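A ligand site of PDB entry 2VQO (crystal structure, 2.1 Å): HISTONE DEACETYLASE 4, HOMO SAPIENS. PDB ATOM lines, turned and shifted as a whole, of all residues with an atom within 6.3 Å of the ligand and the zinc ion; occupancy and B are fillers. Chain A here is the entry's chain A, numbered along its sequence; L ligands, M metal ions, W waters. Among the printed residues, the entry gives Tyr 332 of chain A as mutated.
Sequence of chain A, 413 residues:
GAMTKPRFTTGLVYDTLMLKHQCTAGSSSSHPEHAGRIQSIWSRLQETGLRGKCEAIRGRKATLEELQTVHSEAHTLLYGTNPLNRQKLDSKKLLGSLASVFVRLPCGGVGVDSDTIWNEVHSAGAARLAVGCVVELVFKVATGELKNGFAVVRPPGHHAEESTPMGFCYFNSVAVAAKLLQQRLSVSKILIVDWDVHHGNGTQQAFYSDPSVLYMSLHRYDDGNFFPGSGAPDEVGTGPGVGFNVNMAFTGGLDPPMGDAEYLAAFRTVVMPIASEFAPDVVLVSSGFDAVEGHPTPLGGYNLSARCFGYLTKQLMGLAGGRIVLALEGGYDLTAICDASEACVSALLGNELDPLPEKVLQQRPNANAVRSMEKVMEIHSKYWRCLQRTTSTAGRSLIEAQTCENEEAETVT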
ATOM      1  N   ARG A  37      21.699  21.926   1.964  1.00  0.00           N
ATOM      2  CA  ARG A  37      22.795  21.266   2.701  1.00  0.00           C
ATOM      3  C   ARG A  37      23.662  20.346   1.837  1.00  0.00           C
ATOM      4  O   ARG A  37      24.881  20.521   1.771  1.00  0.00           O
ATOM      5  CB  ARG A  37      22.242  20.470   3.897  1.00  0.00           C
ATOM      6  CG  ARG A  37      21.541  21.313   4.949  1.00  0.00           C
ATOM      7  CD  ARG A  37      21.199  20.501   6.197  1.00  0.00           C
ATOM      8  NE  ARG A  37      20.531  19.248   5.852  1.00  0.00           N
ATOM      9  CZ  ARG A  37      20.971  18.011   6.118  1.00  0.00           C
ATOM     10  NH1 ARG A  37      22.092  17.805   6.799  1.00  0.00           N
ATOM     11  NH2 ARG A  37      20.253  16.968   5.721  1.00  0.00           N
ATOM     12  N   PRO A 156      17.838  12.768   6.600  1.00  0.00           N
ATOM     13  CA  PRO A 156      18.515  11.839   7.504  1.00  0.00           C
ATOM     14  C   PRO A 156      17.627  10.637   7.882  1.00  0.00           C
ATOM     15  O   PRO A 156      16.433  10.617   7.553  1.00  0.00           O
ATOM     16  CB  PRO A 156      18.830  12.714   8.731  1.00  0.00           C
ATOM     17  CG  PRO A 156      17.817  13.771   8.696  1.00  0.00           C
ATOM     18  CD  PRO A 156      17.555  14.058   7.262  1.00  0.00           C
ATOM     19  N   GLY A 157      18.198   9.645   8.569  1.00  0.00           N
ATOM     20  CA  GLY A 157      17.491   8.397   8.818  1.00  0.00           C
ATOM     21  C   GLY A 157      17.395   7.876  10.245  1.00  0.00           C
ATOM     22  O   GLY A 157      16.526   7.050  10.540  1.00  0.00           O
ATOM     23  N   HIS A 158      18.270   8.341  11.130  1.00  0.00           N
ATOM     24  CA  HIS A 158      18.486   7.644  12.410  1.00  0.00           C
ATOM     25  C   HIS A 158      17.359   7.786  13.438  1.00  0.00           C
ATOM     26  O   HIS A 158      17.333   7.029  14.411  1.00  0.00           O
ATOM     27  CB  HIS A 158      19.857   7.974  13.006  1.00  0.00           C
ATOM     28  CG  HIS A 158      19.983   9.356  13.574  1.00  0.00           C
ATOM     29  ND1 HIS A 158      20.831   9.653  14.620  1.00  0.00           N
ATOM     30  CD2 HIS A 158      19.374  10.523  13.251  1.00  0.00           C
ATOM     31  CE1 HIS A 158      20.736  10.936  14.911  1.00  0.00           C
ATOM     32  NE2 HIS A 158      19.859  11.487  14.092  1.00  0.00           N
ATOM     33  N   HIS A 159      16.419   8.695  13.227  1.00  0.00           N
ATOM     34  CA  HIS A 159      15.249   8.802  14.116  1.00  0.00           C
ATOM     35  C   HIS A 159      14.080   7.905  13.690  1.00  0.00           C
ATOM     36  O   HIS A 159      13.187   7.658  14.485  1.00  0.00           O
ATOM     37  CB  HIS A 159      14.753  10.243  14.252  1.00  0.00           C
ATOM     38  CG  HIS A 159      15.734  11.156  14.908  1.00  0.00           C
ATOM     39  ND1 HIS A 159      16.287  10.900  16.142  1.00  0.00           N
ATOM     40  CD2 HIS A 159      16.255  12.335  14.495  1.00  0.00           C
ATOM     41  CE1 HIS A 159      17.108  11.876  16.465  1.00  0.00           C
ATOM     42  NE2 HIS A 159      17.116  12.765  15.484  1.00  0.00           N
ATOM     43  N   MET A 166       9.853  10.202  12.129  1.00  0.00           N
ATOM     44  CA  MET A 166      10.010  11.292  13.087  1.00  0.00           C
ATOM     45  C   MET A 166      11.351  11.994  12.892  1.00  0.00           C
ATOM     46  O   MET A 166      12.247  11.456  12.263  1.00  0.00           O
ATOM     47  CB  MET A 166       9.890  10.777  14.529  1.00  0.00           C
ATOM     48  CG  MET A 166      10.743   9.572  14.851  1.00  0.00           C
ATOM     49  SD  MET A 166      10.674   9.088  16.597  1.00  0.00           S
ATOM     50  CE  MET A 166      11.433  10.507  17.372  1.00  0.00           C
ATOM     51  N   GLY A 167      11.454  13.193  13.446  1.00  0.00           N
ATOM     52  CA  GLY A 167      12.682  13.997  13.360  1.00  0.00           C
ATOM     53  C   GLY A 167      13.221  14.121  11.950  1.00  0.00           C
ATOM     54  O   GLY A 167      14.424  13.945  11.723  1.00  0.00           O
ATOM     55  N   PHE A 168      12.341  14.404  10.993  1.00  0.00           N
ATOM     56  CA  PHE A 168      12.710  14.572   9.572  1.00  0.00           C
ATOM     57  C   PHE A 168      13.110  13.261   8.883  1.00  0.00           C
ATOM     58  O   PHE A 168      13.512  13.286   7.719  1.00  0.00           O
ATOM     59  CB  PHE A 168      13.847  15.599   9.407  1.00  0.00           C
ATOM     60  CG  PHE A 168      13.576  16.927  10.048  1.00  0.00           C
ATOM     61  CD1 PHE A 168      14.273  17.334  11.168  1.00  0.00           C
ATOM     62  CD2 PHE A 168      12.626  17.794   9.513  1.00  0.00           C
ATOM     63  CE1 PHE A 168      14.030  18.569  11.767  1.00  0.00           C
ATOM     64  CE2 PHE A 168      12.372  19.020  10.102  1.00  0.00           C
ATOM     65  CZ  PHE A 168      13.077  19.405  11.232  1.00  0.00           C
ATOM     66  N   CYS A 169      12.966  12.134   9.581  1.00  0.00           N
ATOM     67  CA  CYS A 169      13.404  10.843   9.072  1.00  0.00           C
ATOM     68  C   CYS A 169      12.216   9.974   8.654  1.00  0.00           C
ATOM     69  O   CYS A 169      11.265   9.830   9.400  1.00  0.00           O
ATOM     70  CB  CYS A 169      14.261  10.107  10.115  1.00  0.00           C
ATOM     71  SG  CYS A 169      15.709  11.029  10.706  1.00  0.00           S
ATOM     72  N   ASP A 196      26.006  12.234  15.432  1.00  0.00           N
ATOM     73  CA  ASP A 196      25.004  13.291  15.417  1.00  0.00           C
ATOM     74  C   ASP A 196      24.743  13.691  16.881  1.00  0.00           C
ATOM     75  O   ASP A 196      24.825  12.836  17.769  1.00  0.00           O
ATOM     76  CB  ASP A 196      23.722  12.764  14.757  1.00  0.00           C
ATOM     77  CG  ASP A 196      22.743  13.861  14.373  1.00  0.00           C
ATOM     78  OD1 ASP A 196      22.652  14.180  13.178  1.00  0.00           O
ATOM     79  OD2 ASP A 196      22.054  14.415  15.255  1.00  0.00           O
ATOM     80  N   VAL A 197      24.439  14.952  17.143  1.00  0.00           N
ATOM     81  CA  VAL A 197      24.279  15.402  18.529  1.00  0.00           C
ATOM     82  C   VAL A 197      23.029  14.826  19.223  1.00  0.00           C
ATOM     83  O   VAL A 197      22.909  14.900  20.435  1.00  0.00           O
ATOM     84  CB  VAL A 197      24.320  16.953  18.652  1.00  0.00           C
ATOM     85  CG1 VAL A 197      22.926  17.566  18.421  1.00  0.00           C
ATOM     86  CG2 VAL A 197      24.901  17.378  20.008  1.00  0.00           C
ATOM     87  N   HIS A 198      22.091  14.257  18.452  1.00  0.00           N
ATOM     88  CA  HIS A 198      20.872  13.651  18.997  1.00  0.00           C
ATOM     89  C   HIS A 198      20.970  12.124  19.012  1.00  0.00           C
ATOM     90  O   HIS A 198      21.630  11.536  18.154  1.00  0.00           O
ATOM     91  CB  HIS A 198      19.660  14.112  18.177  1.00  0.00           C
ATOM     92  CG  HIS A 198      19.518  15.607  18.109  1.00  0.00           C
ATOM     93  ND1 HIS A 198      20.049  16.349  17.078  1.00  0.00           N
ATOM     94  CD2 HIS A 198      18.943  16.484  18.949  1.00  0.00           C
ATOM     95  CE1 HIS A 198      19.797  17.628  17.280  1.00  0.00           C
ATOM     96  NE2 HIS A 198      19.125  17.741  18.422  1.00  0.00           N
ATOM     97  N   PHE A 226      16.371  16.245  26.334  1.00  0.00           N
ATOM     98  CA  PHE A 226      16.851  16.680  25.014  1.00  0.00           C
ATOM     99  C   PHE A 226      16.310  15.722  23.946  1.00  0.00           C
ATOM    100  O   PHE A 226      16.224  14.515  24.176  1.00  0.00           O
ATOM    101  CB  PHE A 226      18.387  16.708  24.992  1.00  0.00           C
ATOM    102  CG  PHE A 226      18.962  17.520  23.862  1.00  0.00           C
ATOM    103  CD1 PHE A 226      18.822  18.894  23.842  1.00  0.00           C
ATOM    104  CD2 PHE A 226      19.650  16.902  22.825  1.00  0.00           C
ATOM    105  CE1 PHE A 226      19.347  19.651  22.795  1.00  0.00           C
ATOM    106  CE2 PHE A 226      20.184  17.648  21.777  1.00  0.00           C
ATOM    107  CZ  PHE A 226      20.035  19.023  21.769  1.00  0.00           C
ATOM    108  N   PHE A 227      15.929  16.258  22.790  1.00  0.00           N
ATOM    109  CA  PHE A 227      15.296  15.470  21.739  1.00  0.00           C
ATOM    110  C   PHE A 227      16.208  14.355  21.232  1.00  0.00           C
ATOM    111  O   PHE A 227      17.402  14.592  21.008  1.00  0.00           O
ATOM    112  CB  PHE A 227      14.891  16.391  20.566  1.00  0.00           C
ATOM    113  CG  PHE A 227      14.279  15.655  19.398  1.00  0.00           C
ATOM    114  CD1 PHE A 227      12.903  15.499  19.308  1.00  0.00           C
ATOM    115  CD2 PHE A 227      15.071  15.157  18.375  1.00  0.00           C
ATOM    116  CE1 PHE A 227      12.338  14.842  18.220  1.00  0.00           C
ATOM    117  CE2 PHE A 227      14.508  14.493  17.280  1.00  0.00           C
ATOM    118  CZ  PHE A 227      13.137  14.340  17.203  1.00  0.00           C
ATOM    119  N   PRO A 228      15.666  13.133  21.012  1.00  0.00           N
ATOM    120  CA  PRO A 228      14.266  12.706  21.159  1.00  0.00           C
ATOM    121  C   PRO A 228      13.886  12.174  22.565  1.00  0.00           C
ATOM    122  O   PRO A 228      12.773  11.687  22.733  1.00  0.00           O
ATOM    123  CB  PRO A 228      14.148  11.588  20.125  1.00  0.00           C
ATOM    124  CG  PRO A 228      15.488  10.993  20.073  1.00  0.00           C
ATOM    125  CD  PRO A 228      16.501  12.036  20.521  1.00  0.00           C
ATOM    126  N   GLY A 288      26.279  12.909  11.652  1.00  0.00           N
ATOM    127  CA  GLY A 288      25.627  14.205  11.768  1.00  0.00           C
ATOM    128  C   GLY A 288      26.626  15.193  12.339  1.00  0.00           C
ATOM    129  O   GLY A 288      27.467  14.814  13.148  1.00  0.00           O
ATOM    130  N   ASP A 290      25.707  18.374  13.744  1.00  0.00           N
ATOM    131  CA  ASP A 290      25.037  19.405  14.544  1.00  0.00           C
ATOM    132  C   ASP A 290      25.722  19.678  15.882  1.00  0.00           C
ATOM    133  O   ASP A 290      25.359  20.627  16.571  1.00  0.00           O
ATOM    134  CB  ASP A 290      23.531  19.136  14.716  1.00  0.00           C
ATOM    135  CG  ASP A 290      23.210  17.671  15.001  1.00  0.00           C
ATOM    136  OD1 ASP A 290      24.139  16.877  15.266  1.00  0.00           O
ATOM    137  OD2 ASP A 290      22.011  17.327  14.967  1.00  0.00           O
ATOM    138  N   PRO A 298      18.994  24.851  21.426  1.00  0.00           N
ATOM    139  CA  PRO A 298      18.092  23.686  21.311  1.00  0.00           C
ATOM    140  C   PRO A 298      18.401  22.779  20.111  1.00  0.00           C
ATOM    141  O   PRO A 298      18.301  21.549  20.228  1.00  0.00           O
ATOM    142  CB  PRO A 298      16.707  24.319  21.179  1.00  0.00           C
ATOM    143  CG  PRO A 298      16.931  25.733  20.741  1.00  0.00           C
ATOM    144  CD  PRO A 298      18.395  26.084  20.909  1.00  0.00           C
ATOM    145  N   LEU A 299      18.766  23.347  18.970  1.00  0.00           N
ATOM    146  CA  LEU A 299      19.079  22.553  17.775  1.00  0.00           C
ATOM    147  C   LEU A 299      20.587  22.420  17.630  1.00  0.00           C
ATOM    148  O   LEU A 299      21.153  22.699  16.567  1.00  0.00           O
ATOM    149  CB  LEU A 299      18.459  23.184  16.535  1.00  0.00           C
ATOM    150  CG  LEU A 299      16.929  23.192  16.493  1.00  0.00           C
ATOM    151  CD1 LEU A 299      16.438  24.172  15.436  1.00  0.00           C
ATOM    152  CD2 LEU A 299      16.397  21.798  16.231  1.00  0.00           C
ATOM    153  N   GLU A 329      23.855  12.686   8.446  1.00  0.00           N
ATOM    154  CA  GLU A 329      22.607  12.756   9.187  1.00  0.00           C
ATOM    155  C   GLU A 329      22.220  14.236   9.375  1.00  0.00           C
ATOM    156  O   GLU A 329      21.828  14.898   8.424  1.00  0.00           O
ATOM    157  CB  GLU A 329      22.726  12.022  10.517  1.00  0.00           C
ATOM    158  CG  GLU A 329      22.981  10.522  10.394  1.00  0.00           C
ATOM    159  CD  GLU A 329      21.743   9.712  10.004  1.00  0.00           C
ATOM    160  OE1 GLU A 329      20.660  10.294   9.801  1.00  0.00           O
ATOM    161  OE2 GLU A 329      21.872   8.473   9.897  1.00  0.00           O
ATOM    162  N   GLY A 330      22.354  14.754  10.599  1.00  0.00           N
ATOM    163  CA  GLY A 330      21.991  16.128  10.902  1.00  0.00           C
ATOM    164  C   GLY A 330      23.120  17.119  10.770  1.00  0.00           C
ATOM    165  O   GLY A 330      24.151  16.846  10.150  1.00  0.00           O
ATOM    166  N   GLY A 331      22.928  18.285  11.382  1.00  0.00           N
ATOM    167  CA  GLY A 331      23.760  19.453  11.107  1.00  0.00           C
ATOM    168  C   GLY A 331      23.090  20.227   9.998  1.00  0.00           C
ATOM    169  O   GLY A 331      22.497  19.636   9.097  1.00  0.00           O
ATOM    170  N   TYR A 332      23.143  21.552  10.076  1.00  0.00           N
ATOM    171  CA  TYR A 332      22.435  22.413   9.114  1.00  0.00           C
ATOM    172  C   TYR A 332      23.120  23.747   8.800  1.00  0.00           C
ATOM    173  O   TYR A 332      22.838  24.357   7.761  1.00  0.00           O
ATOM    174  CB  TYR A 332      20.991  22.661   9.585  1.00  0.00           C
ATOM    175  CG  TYR A 332      20.904  23.281  10.955  1.00  0.00           C
ATOM    176  CD1 TYR A 332      20.690  22.490  12.077  1.00  0.00           C
ATOM    177  CD2 TYR A 332      21.028  24.649  11.128  1.00  0.00           C
ATOM    178  CE1 TYR A 332      20.609  23.049  13.336  1.00  0.00           C
ATOM    179  CE2 TYR A 332      20.961  25.220  12.379  1.00  0.00           C
ATOM    180  CZ  TYR A 332      20.745  24.419  13.481  1.00  0.00           C
ATOM    181  OH  TYR A 332      20.680  24.983  14.725  1.00  0.00           O
HETATM  182  C1  LIG L   1      10.509  24.183  17.096  1.00  0.00           C
HETATM  183  C2  LIG L   1      10.421  25.312  17.894  1.00  0.00           C
HETATM  184  C3  LIG L   1      11.539  25.759  18.598  1.00  0.00           C
HETATM  185  C4  LIG L   1      12.741  25.064  18.502  1.00  0.00           C
HETATM  186  C5  LIG L   1      12.830  23.935  17.704  1.00  0.00           C
HETATM  187  C6  LIG L   1      11.714  23.491  16.983  1.00  0.00           C
HETATM  188  C7  LIG L   1      11.754  22.330  16.202  1.00  0.00           C
HETATM  189  C8  LIG L   1      11.208  22.059  15.021  1.00  0.00           C
HETATM  190  N1  LIG L   1      11.496  20.790  14.690  1.00  0.00           N
HETATM  191  C9  LIG L   1      12.220  20.225  15.649  1.00  0.00           C
HETATM  192  C10 LIG L   1      12.785  18.780  15.743  1.00  0.00           C
HETATM  193  N2  LIG L   1      12.397  21.183  16.645  1.00  0.00           N
HETATM  194  C11 LIG L   1      13.159  20.933  17.881  1.00  0.00           C
HETATM  195  C12 LIG L   1      13.353  19.463  18.087  1.00  0.00           C
HETATM  196  N3  LIG L   1      13.766  18.799  16.835  1.00  0.00           N
HETATM  197  C13 LIG L   1      15.017  18.334  16.770  1.00  0.00           C
HETATM  198  O1  LIG L   1      15.687  18.441  17.790  1.00  0.00           O
HETATM  199  C14 LIG L   1      15.668  17.536  15.641  1.00  0.00           C
HETATM  200  S1  LIG L   1      17.308  17.450  15.448  1.00  0.00           S
HETATM  201  C15 LIG L   1      15.091  16.692  14.767  1.00  0.00           C
HETATM  202  C16 LIG L   1      15.975  16.055  13.958  1.00  0.00           C
HETATM  203  C17 LIG L   1      17.266  16.370  14.195  1.00  0.00           C
HETATM  204  C18 LIG L   1      18.534  15.819  13.523  1.00  0.00           C
HETATM  205  C19 LIG L   1      18.282  15.206  12.141  1.00  0.00           C
HETATM  206  F1  LIG L   1      17.727  16.099  11.355  1.00  0.00           F
HETATM  207  F2  LIG L   1      19.440  14.820  11.631  1.00  0.00           F
HETATM  208  F3  LIG L   1      17.485  14.131  12.259  1.00  0.00           F
HETATM  209  O2  LIG L   1      19.052  14.755  14.367  1.00  0.00           O
HETATM  210  O3  LIG L   1      19.582  16.801  13.491  1.00  0.00           O
HETATM  211 ZN    ZN M   1      20.804  15.811  15.182  1.00  0.00          ZN
HETATM  212  O   HOH W   1      19.979  18.796  12.128  1.00  0.00           O
HETATM  213  O   HOH W   2       9.648  19.153  13.732  1.00  0.00           O
HETATM  214  O   HOH W   3      17.026  19.229  20.025  1.00  0.00           O
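N of Gly 330 lies within hydrogen-bond range of OD1 of Asp 196.
The backbone NH (N) of Val 197 sits at hydrogen-bond distance from the side-chain carboxylate (OD1) of Asp 290 (2.7 Å).
A ring nitrogen (NE2) of His 159 sits at hydrogen-bond distance from a ring nitrogen (NE2) of His 158 (3.3 Å).
The side-chain sulfur of Cys 169 lies within hydrogen-bond range of the backbone carbonyl oxygen of Gly 167 (3.3 Å).
O of Pro 156 is in hydrogen-bond range of SG of Cys 169, 3.3 Å away.
The side-chain carboxylate (OE1) of Glu 329 lies within hydrogen-bond range of the backbone NH (N) of Gly 157.
The backbone carbonyl oxygen of Glu 329 sits at hydrogen-bond distance from the guanidinium group of Arg 37 (3.3 Å).
O of Leu 299 is in hydrogen-bond range of OH of Tyr 332 (3.0 Å).
A fluorine (F3) of the ligand sits close to the backbone carbonyl oxygen of Gly 167 (3.1 Å).
The backbone NH (N) of Gly 330 lies close to a fluorine (F2) of the ligand (3.1 Å).
Merely in contact with the ligand: Phe 227, Phe 168, Pro 156, Glu 329, Leu 299 and Cys 169.
13 residues have an atom within 4 Å of the ligand: Pro 156, His 158, His 159, Gly 167, Phe 168, Cys 169, Asp 196, His 198, Phe 227, Asp 290, Leu 299, Glu 329 and Gly 330.
The nearest printed residue that does not touch the ligand is Gly 331 (4.2 Å).
Along chain A the residues within 4 Å of the zinc ion span positions 196 to 290.
An oxygen (O2) of the ligand lies close to a ring nitrogen (NE2) of His 159.
A ring nitrogen (NE2) of His 158 sits close to an oxygen (O2) of the ligand.
Water W3 lies within hydrogen-bond range of the backbone carbonyl oxygen of Pro 298, an oxygen (O1) of the ligand and a ring nitrogen (NE2) of His 198.
The zinc ion is bound by the side-chain carboxylate of Asp 196, the side-chain carboxylate of Asp 290, a ring nitrogen (ND1) of His 198, an oxygen (O2) of the ligand and an oxygen (O3) of the ligand.
The zinc ion has five donor atoms within binding distance.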
